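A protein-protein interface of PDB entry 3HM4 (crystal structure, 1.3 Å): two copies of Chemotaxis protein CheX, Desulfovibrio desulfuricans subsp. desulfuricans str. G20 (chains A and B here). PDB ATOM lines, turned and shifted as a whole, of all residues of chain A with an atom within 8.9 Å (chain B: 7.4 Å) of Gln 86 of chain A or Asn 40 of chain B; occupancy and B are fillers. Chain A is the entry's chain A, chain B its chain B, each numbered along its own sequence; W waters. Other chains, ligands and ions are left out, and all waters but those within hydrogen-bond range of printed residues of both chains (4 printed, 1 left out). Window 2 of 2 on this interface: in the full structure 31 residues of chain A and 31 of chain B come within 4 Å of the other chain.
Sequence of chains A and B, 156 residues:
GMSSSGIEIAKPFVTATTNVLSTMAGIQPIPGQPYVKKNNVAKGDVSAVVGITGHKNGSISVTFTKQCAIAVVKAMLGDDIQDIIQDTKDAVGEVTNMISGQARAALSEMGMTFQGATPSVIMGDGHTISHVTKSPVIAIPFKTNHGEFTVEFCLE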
ATOM      1  N   VAL A  73      13.942 -20.226 -10.168  1.00  0.00           N
ATOM      2  CA  VAL A  73      14.533 -19.637 -11.368  1.00  0.00           C
ATOM      3  C   VAL A  73      14.173 -20.505 -12.605  1.00  0.00           C
ATOM      4  O   VAL A  73      13.790 -19.963 -13.650  1.00  0.00           O
ATOM      5  CB  VAL A  73      16.068 -19.434 -11.239  1.00  0.00           C
ATOM      6  CG1 VAL A  73      16.698 -19.071 -12.596  1.00  0.00           C
ATOM      7  CG2 VAL A  73      16.378 -18.384 -10.159  1.00  0.00           C
ATOM      8  N   LEU A  77      11.840 -18.964 -15.612  1.00  0.00           N
ATOM      9  CA  LEU A  77      12.572 -18.676 -16.818  1.00  0.00           C
ATOM     10  C   LEU A  77      12.957 -19.892 -17.648  1.00  0.00           C
ATOM     11  O   LEU A  77      13.424 -19.698 -18.776  1.00  0.00           O
ATOM     12  CB  LEU A  77      13.775 -17.806 -16.470  1.00  0.00           C
ATOM     13  CG  LEU A  77      13.444 -16.452 -15.813  1.00  0.00           C
ATOM     14  CD1 LEU A  77      14.666 -15.766 -15.200  1.00  0.00           C
ATOM     15  CD2 LEU A  77      12.799 -15.545 -16.868  1.00  0.00           C
ATOM     16  N   ILE A  81      19.064 -23.043 -17.615  1.00  0.00           N
ATOM     17  CA  ILE A  81      19.364 -21.703 -17.027  1.00  0.00           C
ATOM     18  C   ILE A  81      20.423 -20.966 -17.813  1.00  0.00           C
ATOM     19  O   ILE A  81      21.587 -21.386 -17.854  1.00  0.00           O
ATOM     20  CB  ILE A  81      19.764 -21.745 -15.524  1.00  0.00           C
ATOM     21  CG1 ILE A  81      18.600 -22.256 -14.677  1.00  0.00           C
ATOM     22  CG2 ILE A  81      20.160 -20.361 -15.036  1.00  0.00           C
ATOM     23  CD1 ILE A  81      18.943 -22.397 -13.165  1.00  0.00           C
ATOM     24  N   GLN A  82      20.017 -19.821 -18.378  1.00  0.00           N
ATOM     25  CA  GLN A  82      20.914 -19.016 -19.208  1.00  0.00           C
ATOM     26  C   GLN A  82      22.146 -18.459 -18.470  1.00  0.00           C
ATOM     27  O   GLN A  82      23.289 -18.614 -18.922  1.00  0.00           O
ATOM     28  CB  GLN A  82      20.121 -17.882 -19.859  1.00  0.00           C
ATOM     29  CG  GLN A  82      20.908 -17.043 -20.871  1.00  0.00           C
ATOM     30  CD  GLN A  82      19.989 -16.233 -21.769  1.00  0.00           C
ATOM     31  OE1 GLN A  82      18.950 -15.736 -21.325  1.00  0.00           O
ATOM     32  NE2 GLN A  82      20.352 -16.131 -23.064  1.00  0.00           N
ATOM     33  N   ASP A  83      21.908 -17.816 -17.333  1.00  0.00           N
ATOM     34  CA  ASP A  83      22.979 -17.150 -16.578  1.00  0.00           C
ATOM     35  C   ASP A  83      22.414 -17.130 -15.159  1.00  0.00           C
ATOM     36  O   ASP A  83      21.525 -16.342 -14.898  1.00  0.00           O
ATOM     37  CB  ASP A  83      23.149 -15.762 -17.200  1.00  0.00           C
ATOM     38  CG  ASP A  83      24.003 -14.790 -16.406  1.00  0.00           C
ATOM     39  OD1 ASP A  83      24.333 -14.981 -15.221  1.00  0.00           O
ATOM     40  OD2 ASP A  83      24.266 -13.724 -17.004  1.00  0.00           O
ATOM     41  N   ILE A  84      22.927 -17.995 -14.285  1.00  0.00           N
ATOM     42  CA  ILE A  84      22.396 -18.135 -12.938  1.00  0.00           C
ATOM     43  C   ILE A  84      22.376 -16.814 -12.152  1.00  0.00           C
ATOM     44  O   ILE A  84      21.414 -16.568 -11.449  1.00  0.00           O
ATOM     45  CB  ILE A  84      23.118 -19.260 -12.124  1.00  0.00           C
ATOM     46  CG1 ILE A  84      22.330 -19.598 -10.849  1.00  0.00           C
ATOM     47  CG2 ILE A  84      24.569 -18.857 -11.763  1.00  0.00           C
ATOM     48  CD1 ILE A  84      20.884 -20.047 -11.070  1.00  0.00           C
ATOM     49  N   ILE A  85      23.395 -15.971 -12.251  1.00  0.00           N
ATOM     50  CA  ILE A  85      23.419 -14.715 -11.502  1.00  0.00           C
ATOM     51  C   ILE A  85      22.315 -13.745 -11.996  1.00  0.00           C
ATOM     52  O   ILE A  85      21.479 -13.264 -11.214  1.00  0.00           O
ATOM     53  CB  ILE A  85      24.808 -14.039 -11.527  1.00  0.00           C
ATOM     54  CG1 ILE A  85      25.916 -14.967 -10.987  1.00  0.00           C
ATOM     55  CG2 ILE A  85      24.795 -12.722 -10.759  1.00  0.00           C
ATOM     56  CD1 ILE A  85      25.689 -15.565  -9.654  1.00  0.00           C
ATOM     57  N   GLN A  86      22.293 -13.476 -13.297  1.00  0.00           N
ATOM     58  CA  GLN A  86      21.304 -12.571 -13.839  1.00  0.00           C
ATOM     59  C   GLN A  86      19.872 -13.105 -13.656  1.00  0.00           C
ATOM     60  O   GLN A  86      18.954 -12.341 -13.323  1.00  0.00           O
ATOM     61  CB  GLN A  86      21.554 -12.305 -15.331  1.00  0.00           C
ATOM     62  CG  GLN A  86      20.637 -11.265 -15.922  1.00  0.00           C
ATOM     63  CD  GLN A  86      20.896  -9.873 -15.400  1.00  0.00           C
ATOM     64  OE1 GLN A  86      22.043  -9.449 -15.339  1.00  0.00           O
ATOM     65  NE2 GLN A  86      19.830  -9.147 -15.027  1.00  0.00           N
ATOM     66  N   ASP A  87      19.677 -14.398 -13.902  1.00  0.00           N
ATOM     67  CA  ASP A  87      18.344 -14.977 -13.847  1.00  0.00           C
ATOM     68  C   ASP A  87      17.833 -15.053 -12.403  1.00  0.00           C
ATOM     69  O   ASP A  87      16.632 -14.873 -12.188  1.00  0.00           O
ATOM     70  CB  ASP A  87      18.289 -16.332 -14.565  1.00  0.00           C
ATOM     71  CG  ASP A  87      18.558 -16.251 -16.061  1.00  0.00           C
ATOM     72  OD1 ASP A  87      18.493 -15.165 -16.640  1.00  0.00           O
ATOM     73  OD2 ASP A  87      18.862 -17.324 -16.602  1.00  0.00           O
ATOM     74  N   THR A  88      18.739 -15.319 -11.465  1.00  0.00           N
ATOM     75  CA  THR A  88      18.378 -15.293 -10.034  1.00  0.00           C
ATOM     76  C   THR A  88      17.958 -13.881  -9.610  1.00  0.00           C
ATOM     77  O   THR A  88      16.914 -13.709  -8.990  1.00  0.00           O
ATOM     78  CB  THR A  88      19.501 -15.853  -9.123  1.00  0.00           C
ATOM     79  OG1 THR A  88      19.694 -17.206  -9.514  1.00  0.00           O
ATOM     80  CG2 THR A  88      19.126 -15.794  -7.648  1.00  0.00           C
ATOM     81  N   LYS A  89      18.748 -12.882  -9.971  1.00  0.00           N
ATOM     82  CA  LYS A  89      18.414 -11.494  -9.695  1.00  0.00           C
ATOM     83  C   LYS A  89      17.033 -11.162 -10.254  1.00  0.00           C
ATOM     84  O   LYS A  89      16.169 -10.637  -9.549  1.00  0.00           O
ATOM     85  CB  LYS A  89      19.452 -10.573 -10.303  1.00  0.00           C
ATOM     86  CG  LYS A  89      19.159  -9.097 -10.173  1.00  0.00           C
ATOM     87  CD  LYS A  89      20.245  -8.235 -10.832  1.00  0.00           C
ATOM     88  CE  LYS A  89      19.913  -6.768 -10.652  1.00  0.00           C
ATOM     89  NZ  LYS A  89      21.077  -5.912 -10.979  1.00  0.00           N
ATOM     90  N   ASP A  90      16.830 -11.472 -11.532  1.00  0.00           N
ATOM     91  CA  ASP A  90      15.580 -11.127 -12.188  1.00  0.00           C
ATOM     92  C   ASP A  90      14.351 -11.865 -11.640  1.00  0.00           C
ATOM     93  O   ASP A  90      13.306 -11.255 -11.337  1.00  0.00           O
ATOM     94  CB  ASP A  90      15.654 -11.315 -13.712  1.00  0.00           C
ATOM     95  CG  ASP A  90      16.568 -10.310 -14.396  1.00  0.00           C
ATOM     96  OD1 ASP A  90      16.841  -9.213 -13.848  1.00  0.00           O
ATOM     97  OD2 ASP A  90      17.046 -10.639 -15.513  1.00  0.00           O
ATOM     98  N   ALA A  91      14.480 -13.180 -11.483  1.00  0.00           N
ATOM     99  CA  ALA A  91      13.347 -14.023 -11.053  1.00  0.00           C
ATOM    100  C   ALA A  91      12.997 -13.787  -9.584  1.00  0.00           C
ATOM    101  O   ALA A  91      11.843 -13.527  -9.228  1.00  0.00           O
ATOM    102  CB  ALA A  91      13.655 -15.520 -11.280  1.00  0.00           C
ATOM    103  N   VAL A  92      14.010 -13.845  -8.723  1.00  0.00           N
ATOM    104  CA  VAL A  92      13.767 -13.637  -7.284  1.00  0.00           C
ATOM    105  C   VAL A  92      13.392 -12.191  -7.020  1.00  0.00           C
ATOM    106  O   VAL A  92      12.559 -11.921  -6.153  1.00  0.00           O
ATOM    107  CB  VAL A  92      14.945 -14.147  -6.418  1.00  0.00           C
ATOM    108  CG1 VAL A  92      14.747 -13.765  -4.919  1.00  0.00           C
ATOM    109  CG2 VAL A  92      15.105 -15.660  -6.622  1.00  0.00           C
ATOM    110  N   GLY A  93      13.989 -11.274  -7.776  1.00  0.00           N
ATOM    111  CA  GLY A  93      13.628  -9.864  -7.637  1.00  0.00           C
ATOM    112  C   GLY A  93      12.156  -9.615  -7.967  1.00  0.00           C
ATOM    113  O   GLY A  93      11.467  -8.882  -7.249  1.00  0.00           O
ATOM    114  N   GLU A  94      11.662 -10.262  -9.023  1.00  0.00           N
ATOM    115  CA  GLU A  94      10.246 -10.107  -9.361  1.00  0.00           C
ATOM    116  C   GLU A  94       9.339 -10.738  -8.327  1.00  0.00           C
ATOM    117  O   GLU A  94       8.320 -10.161  -7.944  1.00  0.00           O
ATOM    118  CB  GLU A  94       9.950 -10.642 -10.756  1.00  0.00           C
ATOM    119  CG  GLU A  94       8.472 -10.472 -11.166  1.00  0.00           C
ATOM    120  CD  GLU A  94       7.967  -9.001 -11.177  1.00  0.00           C
ATOM    121  OE1 GLU A  94       8.764  -8.057 -11.380  1.00  0.00           O
ATOM    122  OE2 GLU A  94       6.735  -8.776 -11.014  1.00  0.00           O
ATOM    123  N   VAL A 121      18.620  -8.434  -4.005  1.00  0.00           N
ATOM    124  CA  VAL A 121      18.844  -9.871  -4.039  1.00  0.00           C
ATOM    125  C   VAL A 121      20.278 -10.145  -3.629  1.00  0.00           C
ATOM    126  O   VAL A 121      21.224  -9.515  -4.134  1.00  0.00           O
ATOM    127  CB  VAL A 121      18.517 -10.494  -5.417  1.00  0.00           C
ATOM    128  CG1 VAL A 121      18.894 -11.984  -5.387  1.00  0.00           C
ATOM    129  CG2 VAL A 121      17.067 -10.294  -5.776  1.00  0.00           C
ATOM    130  N   ILE A 122      20.435 -11.067  -2.676  1.00  0.00           N
ATOM    131  CA  ILE A 122      21.704 -11.443  -2.108  1.00  0.00           C
ATOM    132  C   ILE A 122      22.045 -12.871  -2.516  1.00  0.00           C
ATOM    133  O   ILE A 122      21.206 -13.770  -2.441  1.00  0.00           O
ATOM    134  CB  ILE A 122      21.682 -11.337  -0.569  1.00  0.00           C
ATOM    135  CG1 ILE A 122      21.438  -9.865  -0.136  1.00  0.00           C
ATOM    136  CG2 ILE A 122      22.994 -11.830   0.072  1.00  0.00           C
ATOM    137  CD1 ILE A 122      20.084  -9.500   0.044  1.00  0.00           C
ATOM    138  N   MET A 123      23.286 -13.090  -2.966  1.00  0.00           N
ATOM    139  CA  MET A 123      23.719 -14.428  -3.296  1.00  0.00           C
ATOM    140  C   MET A 123      25.044 -14.782  -2.645  1.00  0.00           C
ATOM    141  O   MET A 123      25.888 -13.926  -2.414  1.00  0.00           O
ATOM    142  CB  MET A 123      23.842 -14.577  -4.801  1.00  0.00           C
ATOM    143  CG  MET A 123      22.574 -14.245  -5.596  1.00  0.00           C
ATOM    144  SD  MET A 123      22.767 -14.377  -7.483  1.00  0.00           S
ATOM    145  CE  MET A 123      21.797 -12.826  -8.005  1.00  0.00           C
ATOM    146  N   LYS B  37      26.609   2.005 -12.462  1.00  0.00           N
ATOM    147  CA  LYS B  37      27.066   0.610 -12.485  1.00  0.00           C
ATOM    148  C   LYS B  37      26.879  -0.013 -13.879  1.00  0.00           C
ATOM    149  O   LYS B  37      25.842   0.190 -14.488  1.00  0.00           O
ATOM    150  CB  LYS B  37      26.278  -0.266 -11.493  1.00  0.00           C
ATOM    151  CG  LYS B  37      26.494  -0.059 -10.020  1.00  0.00           C
ATOM    152  CD  LYS B  37      25.744  -1.198  -9.255  1.00  0.00           C
ATOM    153  CE  LYS B  37      26.414  -2.578  -9.308  1.00  0.00           C
ATOM    154  NZ  LYS B  37      27.706  -2.713  -8.678  1.00  0.00           N
ATOM    155  N   LYS B  38      27.881  -0.762 -14.315  1.00  0.00           N
ATOM    156  CA  LYS B  38      27.800  -1.574 -15.543  1.00  0.00           C
ATOM    157  C   LYS B  38      27.592  -3.076 -15.238  1.00  0.00           C
ATOM    158  O   LYS B  38      27.228  -3.830 -16.154  1.00  0.00           O
ATOM    159  CB  LYS B  38      29.045  -1.353 -16.412  1.00  0.00           C
ATOM    160  CG  LYS B  38      29.164   0.067 -16.935  1.00  0.00           C
ATOM    161  N   ASN B  39      27.844  -3.502 -13.987  1.00  0.00           N
ATOM    162  CA  ASN B  39      27.661  -4.897 -13.546  1.00  0.00           C
ATOM    163  C   ASN B  39      26.316  -5.072 -12.811  1.00  0.00           C
ATOM    164  O   ASN B  39      25.665  -4.082 -12.414  1.00  0.00           O
ATOM    165  CB  ASN B  39      28.845  -5.385 -12.682  1.00  0.00           C
ATOM    166  CG  ASN B  39      29.156  -4.465 -11.511  1.00  0.00           C
ATOM    167  OD1 ASN B  39      28.690  -3.318 -11.455  1.00  0.00           O
ATOM    168  ND2 ASN B  39      29.975  -4.955 -10.583  1.00  0.00           N
ATOM    169  N   ASN B  40      25.903  -6.329 -12.639  1.00  0.00           N
ATOM    170  CA  ASN B  40      24.617  -6.680 -11.994  1.00  0.00           C
ATOM    171  C   ASN B  40      24.739  -6.968 -10.490  1.00  0.00           C
ATOM    172  O   ASN B  40      23.737  -7.312  -9.894  1.00  0.00           O
ATOM    173  CB  ASN B  40      23.913  -7.857 -12.749  1.00  0.00           C
ATOM    174  CG  ASN B  40      24.725  -9.136 -12.793  1.00  0.00           C
ATOM    175  OD1 ASN B  40      25.783  -9.242 -12.172  1.00  0.00           O
ATOM    176  ND2 ASN B  40      24.258 -10.110 -13.607  1.00  0.00           N
ATOM    177  N   VAL B  41      25.946  -6.848  -9.930  1.00  0.00           N
ATOM    178  CA  VAL B  41      26.232  -7.112  -8.527  1.00  0.00           C
ATOM    179  C   VAL B  41      27.286  -6.163  -7.948  1.00  0.00           C
ATOM    180  O   VAL B  41      28.046  -5.524  -8.688  1.00  0.00           O
ATOM    181  CB  VAL B  41      26.813  -8.546  -8.351  1.00  0.00           C
ATOM    182  CG1 VAL B  41      25.828  -9.645  -8.733  1.00  0.00           C
ATOM    183  CG2 VAL B  41      28.140  -8.734  -9.167  1.00  0.00           C
ATOM    184  N   ALA B  42      27.265  -6.048  -6.623  1.00  0.00           N
ATOM    185  CA  ALA B  42      28.374  -5.538  -5.822  1.00  0.00           C
ATOM    186  C   ALA B  42      28.815  -6.721  -4.963  1.00  0.00           C
ATOM    187  O   ALA B  42      27.998  -7.379  -4.313  1.00  0.00           O
ATOM    188  CB  ALA B  42      27.969  -4.390  -4.956  1.00  0.00           C
ATOM    189  N   THR B 128      27.305 -11.368  -2.909  1.00  0.00           N
ATOM    190  CA  THR B 128      26.880 -10.286  -3.768  1.00  0.00           C
ATOM    191  C   THR B 128      25.520  -9.722  -3.367  1.00  0.00           C
ATOM    192  O   THR B 128      24.669 -10.434  -2.855  1.00  0.00           O
ATOM    193  CB  THR B 128      26.802 -10.704  -5.237  1.00  0.00           C
ATOM    194  OG1 THR B 128      25.875 -11.771  -5.448  1.00  0.00           O
ATOM    195  CG2 THR B 128      28.202 -11.153  -5.756  1.00  0.00           C
ATOM    196  N   ILE B 129      25.358  -8.437  -3.644  1.00  0.00           N
ATOM    197  CA  ILE B 129      24.084  -7.751  -3.517  1.00  0.00           C
ATOM    198  C   ILE B 129      23.774  -7.089  -4.855  1.00  0.00           C
ATOM    199  O   ILE B 129      24.656  -6.462  -5.471  1.00  0.00           O
ATOM    200  CB  ILE B 129      24.064  -6.722  -2.353  1.00  0.00           C
ATOM    201  CG1 ILE B 129      22.657  -6.087  -2.211  1.00  0.00           C
ATOM    202  CG2 ILE B 129      25.157  -5.694  -2.489  1.00  0.00           C
ATOM    203  CD1 ILE B 129      22.419  -5.340  -0.879  1.00  0.00           C
ATOM    204  N   SER B 130      22.515  -7.210  -5.263  1.00  0.00           N
ATOM    205  CA  SER B 130      22.020  -6.653  -6.503  1.00  0.00           C
ATOM    206  C   SER B 130      20.742  -5.864  -6.221  1.00  0.00           C
ATOM    207  O   SER B 130      19.837  -6.390  -5.620  1.00  0.00           O
ATOM    208  CB  SER B 130      21.655  -7.778  -7.486  1.00  0.00           C
ATOM    209  OG  SER B 130      22.762  -8.630  -7.799  1.00  0.00           O
ATOM    210  N   HIS B 131      20.677  -4.650  -6.738  1.00  0.00           N
ATOM    211  CA  HIS B 131      19.468  -3.836  -6.688  1.00  0.00           C
ATOM    212  C   HIS B 131      18.527  -4.193  -7.824  1.00  0.00           C
ATOM    213  O   HIS B 131      18.947  -4.280  -8.983  1.00  0.00           O
ATOM    214  CB  HIS B 131      19.811  -2.343  -6.753  1.00  0.00           C
ATOM    215  CG  HIS B 131      20.466  -1.869  -5.505  1.00  0.00           C
ATOM    216  ND1 HIS B 131      19.724  -1.434  -4.434  1.00  0.00           N
ATOM    217  CD2 HIS B 131      21.772  -1.741  -5.152  1.00  0.00           C
ATOM    218  CE1 HIS B 131      20.550  -1.086  -3.456  1.00  0.00           C
ATOM    219  NE2 HIS B 131      21.797  -1.272  -3.865  1.00  0.00           N
HETATM  220  O   HOH W   1      19.009  -3.628 -11.509  1.00  0.00           O
HETATM  221  O   HOH W   2      23.251  -3.397 -11.052  1.00  0.00           O
HETATM  222  O   HOH W   3      25.764 -12.361 -14.712  1.00  0.00           O
HETATM  223  O   HOH W   4      23.413 -10.579  -5.728  1.00  0.00           O
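The side-chain amide oxygen (OE1) of Gln 86 of chain A lies within hydrogen-bond range of the side-chain amide nitrogen (ND2) of Asn 40 of chain B, 2.9 Å away.
The side-chain amino group (NZ) of Lys 89 of chain A is in hydrogen-bond range of the backbone carbonyl oxygen (O) of Asn 40 of chain B (3.2 Å).
The side-chain amino group (NZ) of Lys 89 of chain A sits close to the backbone carbonyl oxygen (O) of His 131 of chain B (3.3 Å).
The backbone NH (N) of Ser 130 of chain B sits at hydrogen-bond distance from the backbone carbonyl oxygen (O) of Val 121 of chain A, at 2.9 Å.
N of Thr 128 of chain B is in hydrogen-bond range of O of Met 123 of chain A.
Of chain B, only Asn 40 (2.9 Å) comes within 4 Å of Gln 86 of chain A.
Asn 40 of chain B touches just these residues of chain A: Ile 85, Gln 86 and Lys 89.
Val 41 of chain B touches just one residue of chain A: Ile 85 (3.8 Å).
Of the printed residues of chain A, Thr 128 of chain B touches Val 121 (3.8 Å), Ile 122 (3.2 Å) and Met 123 (3.0 Å).
Of the printed residues of chain A, Ser 130 of chain B touches Lys 89 (3.7 Å) and Val 121 (2.9 Å).
Of the printed residues of chain A, His 131 of chain B touches Lys 89 (3.1 Å).
The nearest printed residue of chain B that does not touch Gln 86 of chain A is Asn 39 of chain B (6.6 Å).
The nearest residue of chain A that does not touch Asn 40 of chain B is Asp 83 of chain A (5.0 Å).
The nearest printed residue of chain A that does not touch Thr 128 of chain B is Ile 85 of chain A (5.5 Å).
No position is printed for both chains.
Printed residues of chain B that touch a printed residue of chain A: Asn 40, Val 41, Thr 128, Ile 129, Ser 130 and His 131.
Of the 19 printed residues of chain A, 6 touch a printed residue of chain B.
Printed residues of chain A that touch a printed residue of chain B: Ile 85, Gln 86, Lys 89, Val 121, Ile 122 and Met 123.
Hydrophobic or aromatic side chains of chain A within 4 Å of the printed part of chain B: Ile 85, Ile 122 and Met 123.
Along chain A the printed residues that touch a printed residue of chain B span positions 85 to 123.
Water W1 bridges O of His 131 of chain B (2.6 Å) and NZ of Lys 89 of chain A (3.1 Å).
Water W4 lies within hydrogen-bond range of the side-chain hydroxyl of Thr 128 of chain B (2.7 Å), the backbone carbonyl oxygen of Val 121 of chain A (2.9 Å) and the side-chain hydroxyl of Ser 130 of chain B (2.9 Å).
Water W2 lies within hydrogen-bond range of the backbone carbonyl oxygen of Asn 39 of chain B and the side-chain amino group of Lys 89 of chain A.
Water W3 bridges the side-chain amide nitrogen of Asn 40 of chain B and the side-chain carboxylate of Asp 83 of chain A.
Asn 40 of chain B touches Ile 85 of chain A (OD1 to CG2, 3.9 Å).
Ile 85 of chain A touches Val 41 of chain B.
Lys 89 of chain A touches Ser 130 of chain B.
Thr 128 of chain B touches Val 121 of chain A.
Val 121 of chain A touches Ile 129 of chain B (O to CA, 3.4 Å).
Ile 122 of chain A touches Thr 128 of chain B.
OD1 of Asp 83 of chain A lies within hydrogen-bond range of N of Ile 85 of chain A (3.3 Å).
The side-chain carboxylate (OD1) of Asp 83 of chain A lies within hydrogen-bond range of the backbone NH (N) of Gln 86 of chain A (3.2 Å).
The side-chain amide nitrogen of Gln 86 of chain A sits at hydrogen-bond distance from the side-chain carboxylate of Asp 90 of chain A.
The backbone carbonyl oxygen (O) of Val 41 of chain B is in hydrogen-bond range of the side-chain amino group (NZ) of Lys 37 of chain B, 2.8 Å away.
ND2 of Asn 39 of chain B lies within hydrogen-bond range of O of Val 41 of chain B, 2.8 Å away.
The backbone carbonyl oxygen of Asn 40 of chain B lies within hydrogen-bond range of the side-chain hydroxyl of Ser 130 of chain B, at 2.7 Å.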
